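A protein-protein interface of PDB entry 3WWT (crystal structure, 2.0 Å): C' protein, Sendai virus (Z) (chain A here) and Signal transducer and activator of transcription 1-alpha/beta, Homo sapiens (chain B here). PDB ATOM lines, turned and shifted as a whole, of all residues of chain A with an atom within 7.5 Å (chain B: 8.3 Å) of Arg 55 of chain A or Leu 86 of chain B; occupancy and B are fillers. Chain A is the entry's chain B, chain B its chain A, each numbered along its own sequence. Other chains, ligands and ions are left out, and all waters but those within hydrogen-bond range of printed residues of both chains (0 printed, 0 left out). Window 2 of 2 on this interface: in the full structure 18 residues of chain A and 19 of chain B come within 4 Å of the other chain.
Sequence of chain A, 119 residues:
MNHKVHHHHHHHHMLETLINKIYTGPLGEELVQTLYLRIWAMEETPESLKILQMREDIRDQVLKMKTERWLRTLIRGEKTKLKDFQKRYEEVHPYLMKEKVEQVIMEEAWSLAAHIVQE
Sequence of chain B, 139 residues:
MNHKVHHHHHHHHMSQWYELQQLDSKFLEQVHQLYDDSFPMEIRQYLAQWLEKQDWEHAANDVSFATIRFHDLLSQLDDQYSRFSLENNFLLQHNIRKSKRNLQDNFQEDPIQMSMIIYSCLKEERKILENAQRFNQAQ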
ATOM      1  N   LYS A  50       6.068  20.267  -5.947  1.00  0.00           N
ATOM      2  CA  LYS A  50       6.601  20.982  -4.791  1.00  0.00           C
ATOM      3  C   LYS A  50       6.303  22.476  -4.881  1.00  0.00           C
ATOM      4  O   LYS A  50       6.041  23.116  -3.855  1.00  0.00           O
ATOM      5  CB  LYS A  50       8.103  20.715  -4.628  1.00  0.00           C
ATOM      6  CG  LYS A  50       8.996  21.262  -5.722  1.00  0.00           C
ATOM      7  CD  LYS A  50      10.456  21.359  -5.256  1.00  0.00           C
ATOM      8  CE  LYS A  50      11.390  20.504  -6.126  1.00  0.00           C
ATOM      9  NZ  LYS A  50      12.770  21.071  -6.217  1.00  0.00           N
ATOM     10  N   ILE A  51       6.286  23.041  -6.090  1.00  0.00           N
ATOM     11  CA  ILE A  51       5.873  24.431  -6.237  1.00  0.00           C
ATOM     12  C   ILE A  51       4.394  24.586  -5.915  1.00  0.00           C
ATOM     13  O   ILE A  51       3.987  25.553  -5.259  1.00  0.00           O
ATOM     14  CB  ILE A  51       6.205  24.946  -7.643  1.00  0.00           C
ATOM     15  CG1 ILE A  51       7.713  25.196  -7.736  1.00  0.00           C
ATOM     16  CG2 ILE A  51       5.443  26.239  -7.925  1.00  0.00           C
ATOM     17  CD1 ILE A  51       8.099  26.070  -8.864  1.00  0.00           C
ATOM     18  N   LEU A  52       3.562  23.645  -6.373  1.00  0.00           N
ATOM     19  CA  LEU A  52       2.141  23.755  -6.088  1.00  0.00           C
ATOM     20  C   LEU A  52       1.852  23.582  -4.605  1.00  0.00           C
ATOM     21  O   LEU A  52       0.826  24.064  -4.129  1.00  0.00           O
ATOM     22  CB  LEU A  52       1.360  22.729  -6.909  1.00  0.00           C
ATOM     23  CG  LEU A  52       1.352  22.981  -8.415  1.00  0.00           C
ATOM     24  CD1 LEU A  52       0.732  21.796  -9.152  1.00  0.00           C
ATOM     25  CD2 LEU A  52       0.610  24.271  -8.748  1.00  0.00           C
ATOM     26  N   GLN A  53       2.746  22.945  -3.862  1.00  0.00           N
ATOM     27  CA  GLN A  53       2.528  22.701  -2.447  1.00  0.00           C
ATOM     28  C   GLN A  53       3.123  23.788  -1.558  1.00  0.00           C
ATOM     29  O   GLN A  53       2.937  23.738  -0.337  1.00  0.00           O
ATOM     30  CB  GLN A  53       3.104  21.332  -2.067  1.00  0.00           C
ATOM     31  CG  GLN A  53       2.258  20.152  -2.570  1.00  0.00           C
ATOM     32  CD  GLN A  53       3.065  18.873  -2.756  1.00  0.00           C
ATOM     33  OE1 GLN A  53       4.187  18.760  -2.261  1.00  0.00           O
ATOM     34  NE2 GLN A  53       2.494  17.904  -3.477  1.00  0.00           N
ATOM     35  N   MET A  54       3.829  24.758  -2.131  1.00  0.00           N
ATOM     36  CA  MET A  54       4.461  25.792  -1.324  1.00  0.00           C
ATOM     37  C   MET A  54       3.425  26.728  -0.738  1.00  0.00           C
ATOM     38  O   MET A  54       2.403  27.021  -1.365  1.00  0.00           O
ATOM     39  CB  MET A  54       5.430  26.622  -2.154  1.00  0.00           C
ATOM     40  CG  MET A  54       6.771  25.985  -2.354  1.00  0.00           C
ATOM     41  SD  MET A  54       7.731  26.954  -3.515  1.00  0.00           S
ATOM     42  CE  MET A  54       8.183  28.306  -2.535  1.00  0.00           C
ATOM     43  N   ARG A  55       3.711  27.220   0.469  1.00  0.00           N
ATOM     44  CA  ARG A  55       2.926  28.323   1.004  1.00  0.00           C
ATOM     45  C   ARG A  55       2.910  29.458  -0.003  1.00  0.00           C
ATOM     46  O   ARG A  55       3.882  29.686  -0.728  1.00  0.00           O
ATOM     47  CB  ARG A  55       3.489  28.807   2.341  1.00  0.00           C
ATOM     48  CG  ARG A  55       2.404  29.274   3.297  1.00  0.00           C
ATOM     49  CD  ARG A  55       2.983  29.672   4.636  1.00  0.00           C
ATOM     50  NE  ARG A  55       3.925  30.778   4.515  1.00  0.00           N
ATOM     51  CZ  ARG A  55       4.930  30.978   5.360  1.00  0.00           C
ATOM     52  NH1 ARG A  55       5.112  30.139   6.371  1.00  0.00           N
ATOM     53  NH2 ARG A  55       5.754  32.004   5.189  1.00  0.00           N
ATOM     54  N   GLU A  56       1.781  30.166  -0.058  1.00  0.00           N
ATOM     55  CA  GLU A  56       1.508  31.031  -1.200  1.00  0.00           C
ATOM     56  C   GLU A  56       2.506  32.175  -1.302  1.00  0.00           C
ATOM     57  O   GLU A  56       2.912  32.550  -2.407  1.00  0.00           O
ATOM     58  CB  GLU A  56       0.078  31.581  -1.118  1.00  0.00           C
ATOM     59  CG  GLU A  56      -0.113  32.881  -1.888  1.00  0.00           C
ATOM     60  CD  GLU A  56      -1.574  33.227  -2.141  1.00  0.00           C
ATOM     61  OE1 GLU A  56      -2.455  32.404  -1.786  1.00  0.00           O
ATOM     62  OE2 GLU A  56      -1.835  34.318  -2.704  1.00  0.00           O
ATOM     63  N   ASP A  57       2.888  32.774  -0.169  1.00  0.00           N
ATOM     64  CA  ASP A  57       3.818  33.896  -0.245  1.00  0.00           C
ATOM     65  C   ASP A  57       5.207  33.423  -0.654  1.00  0.00           C
ATOM     66  O   ASP A  57       5.912  34.117  -1.390  1.00  0.00           O
ATOM     67  CB  ASP A  57       3.878  34.650   1.088  1.00  0.00           C
ATOM     68  CG  ASP A  57       4.326  33.778   2.231  1.00  0.00           C
ATOM     69  OD1 ASP A  57       3.741  32.690   2.420  1.00  0.00           O
ATOM     70  OD2 ASP A  57       5.278  34.174   2.940  1.00  0.00           O
ATOM     71  N   ILE A  58       5.611  32.240  -0.192  1.00  0.00           N
ATOM     72  CA  ILE A  58       6.912  31.713  -0.588  1.00  0.00           C
ATOM     73  C   ILE A  58       6.894  31.333  -2.061  1.00  0.00           C
ATOM     74  O   ILE A  58       7.824  31.656  -2.806  1.00  0.00           O
ATOM     75  CB  ILE A  58       7.309  30.534   0.311  1.00  0.00           C
ATOM     76  CG1 ILE A  58       7.175  30.920   1.778  1.00  0.00           C
ATOM     77  CG2 ILE A  58       8.751  30.154   0.096  1.00  0.00           C
ATOM     78  CD1 ILE A  58       7.364  29.735   2.706  1.00  0.00           C
ATOM     79  N   ARG A  59       5.814  30.687  -2.519  1.00  0.00           N
ATOM     80  CA  ARG A  59       5.705  30.378  -3.942  1.00  0.00           C
ATOM     81  C   ARG A  59       5.834  31.628  -4.791  1.00  0.00           C
ATOM     82  O   ARG A  59       6.541  31.625  -5.806  1.00  0.00           O
ATOM     83  CB  ARG A  59       4.387  29.677  -4.245  1.00  0.00           C
ATOM     84  CG  ARG A  59       4.259  29.325  -5.728  1.00  0.00           C
ATOM     85  CD  ARG A  59       2.990  28.544  -6.005  1.00  0.00           C
ATOM     86  NE  ARG A  59       1.797  29.266  -5.571  1.00  0.00           N
ATOM     87  CZ  ARG A  59       0.941  28.788  -4.677  1.00  0.00           C
ATOM     88  NH1 ARG A  59       1.161  27.591  -4.126  1.00  0.00           N
ATOM     89  NH2 ARG A  59      -0.125  29.496  -4.342  1.00  0.00           N
ATOM     90  N   ASP A  60       5.171  32.715  -4.388  1.00  0.00           N
ATOM     91  CA  ASP A  60       5.269  33.964  -5.140  1.00  0.00           C
ATOM     92  C   ASP A  60       6.718  34.422  -5.259  1.00  0.00           C
ATOM     93  O   ASP A  60       7.170  34.822  -6.339  1.00  0.00           O
ATOM     94  CB  ASP A  60       4.425  35.064  -4.470  1.00  0.00           C
ATOM     95  CG  ASP A  60       2.935  34.956  -4.803  1.00  0.00           C
ATOM     96  OD1 ASP A  60       2.553  33.996  -5.517  1.00  0.00           O
ATOM     97  OD2 ASP A  60       2.159  35.833  -4.350  1.00  0.00           O
ATOM     98  N   GLN A  61       7.444  34.415  -4.141  1.00  0.00           N
ATOM     99  CA  GLN A  61       8.835  34.863  -4.143  1.00  0.00           C
ATOM    100  C   GLN A  61       9.695  33.994  -5.066  1.00  0.00           C
ATOM    101  O   GLN A  61      10.427  34.512  -5.913  1.00  0.00           O
ATOM    102  CB  GLN A  61       9.376  34.847  -2.707  1.00  0.00           C
ATOM    103  CG  GLN A  61       8.715  35.884  -1.805  1.00  0.00           C
ATOM    104  CD  GLN A  61       8.910  35.610  -0.315  1.00  0.00           C
ATOM    105  OE1 GLN A  61       9.433  34.572   0.083  1.00  0.00           O
ATOM    106  NE2 GLN A  61       8.468  36.547   0.513  1.00  0.00           N
ATOM    107  N   ASP B  79      15.713  26.417  -3.917  1.00  0.00           N
ATOM    108  CA  ASP B  79      15.236  25.471  -2.913  1.00  0.00           C
ATOM    109  C   ASP B  79      15.685  25.886  -1.521  1.00  0.00           C
ATOM    110  O   ASP B  79      14.923  25.768  -0.554  1.00  0.00           O
ATOM    111  CB  ASP B  79      15.737  24.056  -3.215  1.00  0.00           C
ATOM    112  CG  ASP B  79      15.057  23.443  -4.426  1.00  0.00           C
ATOM    113  OD1 ASP B  79      14.005  23.976  -4.861  1.00  0.00           O
ATOM    114  OD2 ASP B  79      15.577  22.432  -4.951  1.00  0.00           O
ATOM    115  N   GLN B  80      16.932  26.358  -1.401  1.00  0.00           N
ATOM    116  CA  GLN B  80      17.414  26.888  -0.124  1.00  0.00           C
ATOM    117  C   GLN B  80      16.592  28.091   0.315  1.00  0.00           C
ATOM    118  O   GLN B  80      16.194  28.201   1.482  1.00  0.00           O
ATOM    119  CB  GLN B  80      18.886  27.278  -0.242  1.00  0.00           C
ATOM    120  CG  GLN B  80      19.816  26.109  -0.103  1.00  0.00           C
ATOM    121  CD  GLN B  80      19.537  25.298   1.135  1.00  0.00           C
ATOM    122  OE1 GLN B  80      19.229  24.107   1.061  1.00  0.00           O
ATOM    123  NE2 GLN B  80      19.642  25.939   2.290  1.00  0.00           N
ATOM    124  N   TYR B  81      16.342  29.012  -0.613  1.00  0.00           N
ATOM    125  CA  TYR B  81      15.518  30.171  -0.313  1.00  0.00           C
ATOM    126  C   TYR B  81      14.168  29.774   0.278  1.00  0.00           C
ATOM    127  O   TYR B  81      13.715  30.365   1.265  1.00  0.00           O
ATOM    128  CB  TYR B  81      15.324  31.005  -1.577  1.00  0.00           C
ATOM    129  CG  TYR B  81      14.502  32.251  -1.345  1.00  0.00           C
ATOM    130  CD1 TYR B  81      13.110  32.204  -1.375  1.00  0.00           C
ATOM    131  CD2 TYR B  81      15.113  33.475  -1.095  1.00  0.00           C
ATOM    132  CE1 TYR B  81      12.352  33.336  -1.159  1.00  0.00           C
ATOM    133  CE2 TYR B  81      14.358  34.625  -0.894  1.00  0.00           C
ATOM    134  CZ  TYR B  81      12.976  34.544  -0.920  1.00  0.00           C
ATOM    135  OH  TYR B  81      12.210  35.669  -0.717  1.00  0.00           O
ATOM    136  N   SER B  82      13.501  28.776  -0.310  1.00  0.00           N
ATOM    137  CA  SER B  82      12.182  28.409   0.201  1.00  0.00           C
ATOM    138  C   SER B  82      12.268  27.832   1.610  1.00  0.00           C
ATOM    139  O   SER B  82      11.347  28.030   2.413  1.00  0.00           O
ATOM    140  CB  SER B  82      11.478  27.436  -0.761  1.00  0.00           C
ATOM    141  OG  SER B  82      12.145  26.193  -0.829  1.00  0.00           O
ATOM    142  N   ARG B  83      13.369  27.157   1.952  1.00  0.00           N
ATOM    143  CA  ARG B  83      13.541  26.692   3.328  1.00  0.00           C
ATOM    144  C   ARG B  83      13.742  27.862   4.293  1.00  0.00           C
ATOM    145  O   ARG B  83      13.075  27.941   5.331  1.00  0.00           O
ATOM    146  CB  ARG B  83      14.709  25.708   3.417  1.00  0.00           C
ATOM    147  CG  ARG B  83      14.601  24.522   2.476  1.00  0.00           C
ATOM    148  CD  ARG B  83      15.486  23.376   2.968  1.00  0.00           C
ATOM    149  NE  ARG B  83      16.046  22.575   1.876  1.00  0.00           N
ATOM    150  CZ  ARG B  83      15.856  21.265   1.731  1.00  0.00           C
ATOM    151  NH1 ARG B  83      15.116  20.592   2.608  1.00  0.00           N
ATOM    152  NH2 ARG B  83      16.414  20.620   0.712  1.00  0.00           N
ATOM    153  N   PHE B  84      14.650  28.793   3.965  1.00  0.00           N
ATOM    154  CA  PHE B  84      14.861  29.958   4.827  1.00  0.00           C
ATOM    155  C   PHE B  84      13.599  30.805   4.953  1.00  0.00           C
ATOM    156  O   PHE B  84      13.353  31.406   6.004  1.00  0.00           O
ATOM    157  CB  PHE B  84      16.016  30.814   4.290  1.00  0.00           C
ATOM    158  CG  PHE B  84      17.380  30.185   4.475  1.00  0.00           C
ATOM    159  CD1 PHE B  84      17.759  29.667   5.708  1.00  0.00           C
ATOM    160  CD2 PHE B  84      18.279  30.111   3.413  1.00  0.00           C
ATOM    161  CE1 PHE B  84      19.017  29.085   5.882  1.00  0.00           C
ATOM    162  CE2 PHE B  84      19.543  29.531   3.575  1.00  0.00           C
ATOM    163  CZ  PHE B  84      19.909  29.012   4.812  1.00  0.00           C
ATOM    164  N   SER B  85      12.807  30.891   3.885  1.00  0.00           N
ATOM    165  CA  SER B  85      11.534  31.604   3.943  1.00  0.00           C
ATOM    166  C   SER B  85      10.576  30.961   4.938  1.00  0.00           C
ATOM    167  O   SER B  85       9.889  31.660   5.701  1.00  0.00           O
ATOM    168  CB  SER B  85      10.905  31.639   2.548  1.00  0.00           C
ATOM    169  OG  SER B  85      11.504  32.628   1.753  1.00  0.00           O
ATOM    170  N   LEU B  86      10.482  29.629   4.907  1.00  0.00           N
ATOM    171  CA  LEU B  86       9.660  28.917   5.875  1.00  0.00           C
ATOM    172  C   LEU B  86      10.109  29.193   7.298  1.00  0.00           C
ATOM    173  O   LEU B  86       9.281  29.212   8.215  1.00  0.00           O
ATOM    174  CB  LEU B  86       9.722  27.421   5.595  1.00  0.00           C
ATOM    175  CG  LEU B  86       8.576  26.763   4.831  1.00  0.00           C
ATOM    176  CD1 LEU B  86       8.755  25.254   4.871  1.00  0.00           C
ATOM    177  CD2 LEU B  86       7.221  27.172   5.402  1.00  0.00           C
ATOM    178  N   GLU B  87      11.418  29.352   7.502  1.00  0.00           N
ATOM    179  CA  GLU B  87      12.031  29.669   8.786  1.00  0.00           C
ATOM    180  C   GLU B  87      11.948  31.154   9.133  1.00  0.00           C
ATOM    181  O   GLU B  87      12.504  31.558  10.159  1.00  0.00           O
ATOM    182  CB  GLU B  87      13.504  29.219   8.774  1.00  0.00           C
ATOM    183  CG  GLU B  87      13.713  27.689   8.870  1.00  0.00           C
ATOM    184  CD  GLU B  87      15.012  27.181   8.220  1.00  0.00           C
ATOM    185  OE1 GLU B  87      15.797  27.991   7.687  1.00  0.00           O
ATOM    186  OE2 GLU B  87      15.257  25.953   8.255  1.00  0.00           O
ATOM    187  N   ASN B  88      11.295  31.966   8.294  1.00  0.00           N
ATOM    188  CA  ASN B  88      11.149  33.416   8.500  1.00  0.00           C
ATOM    189  C   ASN B  88      12.496  34.126   8.646  1.00  0.00           C
ATOM    190  O   ASN B  88      12.644  35.055   9.443  1.00  0.00           O
ATOM    191  CB  ASN B  88      10.254  33.717   9.705  1.00  0.00           C
ATOM    192  CG  ASN B  88       8.879  33.118   9.565  1.00  0.00           C
ATOM    193  OD1 ASN B  88       8.085  33.549   8.730  1.00  0.00           O
ATOM    194  ND2 ASN B  88       8.588  32.112  10.376  1.00  0.00           N
ATOM    195  N   ASN B  89      13.481  33.718   7.852  1.00  0.00           N
ATOM    196  CA  ASN B  89      14.848  34.229   7.972  1.00  0.00           C
ATOM    197  C   ASN B  89      15.083  35.236   6.853  1.00  0.00           C
ATOM    198  O   ASN B  89      15.597  34.900   5.782  1.00  0.00           O
ATOM    199  CB  ASN B  89      15.850  33.081   7.931  1.00  0.00           C
ATOM    200  CG  ASN B  89      17.229  33.485   8.439  1.00  0.00           C
ATOM    201  OD1 ASN B  89      17.679  34.621   8.241  1.00  0.00           O
ATOM    202  ND2 ASN B  89      17.909  32.547   9.087  1.00  0.00           N
ATOM    203  N   GLN B  93      17.203  34.989   3.252  1.00  0.00           N
ATOM    204  CA  GLN B  93      16.439  35.181   2.024  1.00  0.00           C
ATOM    205  C   GLN B  93      17.113  36.217   1.162  1.00  0.00           C
ATOM    206  O   GLN B  93      17.315  36.010  -0.037  1.00  0.00           O
ATOM    207  CB  GLN B  93      15.002  35.626   2.338  1.00  0.00           C
ATOM    208  CG  GLN B  93      14.139  34.589   2.972  1.00  0.00           C
ATOM    209  CD  GLN B  93      12.758  35.139   3.262  1.00  0.00           C
ATOM    210  OE1 GLN B  93      11.972  35.378   2.347  1.00  0.00           O
ATOM    211  NE2 GLN B  93      12.463  35.365   4.539  1.00  0.00           N
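The side-chain amino group of Lys 50 of chain A is in salt-bridge range of the side-chain carboxylate of Asp 79 of chain B (3.4 Å). OE1 of Gln 93 of chain B sits close to OE1 of Gln 61 of chain A (3.5 Å). OG of Ser 85 of chain B lies within hydrogen-bond range of OE1 of Gln 61 of chain A (3.3 Å). OH of Tyr 81 of chain B sits at hydrogen-bond distance from OE1 of Gln 61 of chain A (3.1 Å).
Of the printed residues of chain B, Lys 50 of chain A touches Asp 79. Arg 55 of chain A touches just one residue of chain B: Leu 86 (3.8 Å). Of the printed residues of chain A, Ser 85 of chain B touches Ile 58 (3.6 Å) and Gln 61 (3.3 Å). Leu 86 of chain B touches two residues of chain A. The nearest residue of chain B that does not touch Arg 55 of chain A is Ser 85 of chain B (4.2 Å). The nearest residue of chain A that does not touch Leu 86 of chain B is Gln 61 of chain A (7.0 Å). The nearest printed residue of chain B that does not touch Gln 61 of chain A is Ser 82 of chain B (6.7 Å).
Among the printed residues, pairs that only touch across the chains: Ile 58 of chain A with Ser 85 of chain B, Ile 58 of chain A with Leu 86 of chain B, Arg 55 of chain A with Leu 86 of chain B, Met 54 of chain A with Ser 82 of chain B and Ile 58 of chain A with Ser 82 of chain B.
The backbone carbonyl oxygen (O) of Tyr 81 of chain B lies close to the side-chain hydroxyl (OG) of Ser 85 of chain B, at 3.2 Å. O of Asn 89 of chain B lies close to NE2 of Gln 93 of chain B (3.4 Å). The backbone carbonyl oxygen (O) of Asp 79 of chain B is in hydrogen-bond range of the side-chain hydroxyl (OG) of Ser 82 of chain B, at 2.8 Å. The side-chain hydroxyl of Tyr 81 of chain B lies within hydrogen-bond range of the side-chain amide oxygen of Gln 93 of chain B (3.1 Å). The guanidinium group of Arg 59 of chain A sits at hydrogen-bond distance from the backbone carbonyl oxygen of Met 54 of chain A. OE1 of Gln 93 of chain B is in hydrogen-bond range of OG of Ser 85 of chain B (2.9 Å).
Hydrophobic or aromatic side chains of chain A within 4 Å of the printed part of chain B: Met 54 and Ile 58. Printed residues of chain B that touch a printed residue of chain A: Asp 79, Tyr 81, Ser 82, Ser 85, Leu 86 and Gln 93. Among the printed residues, 9 pairs touch across the chains.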
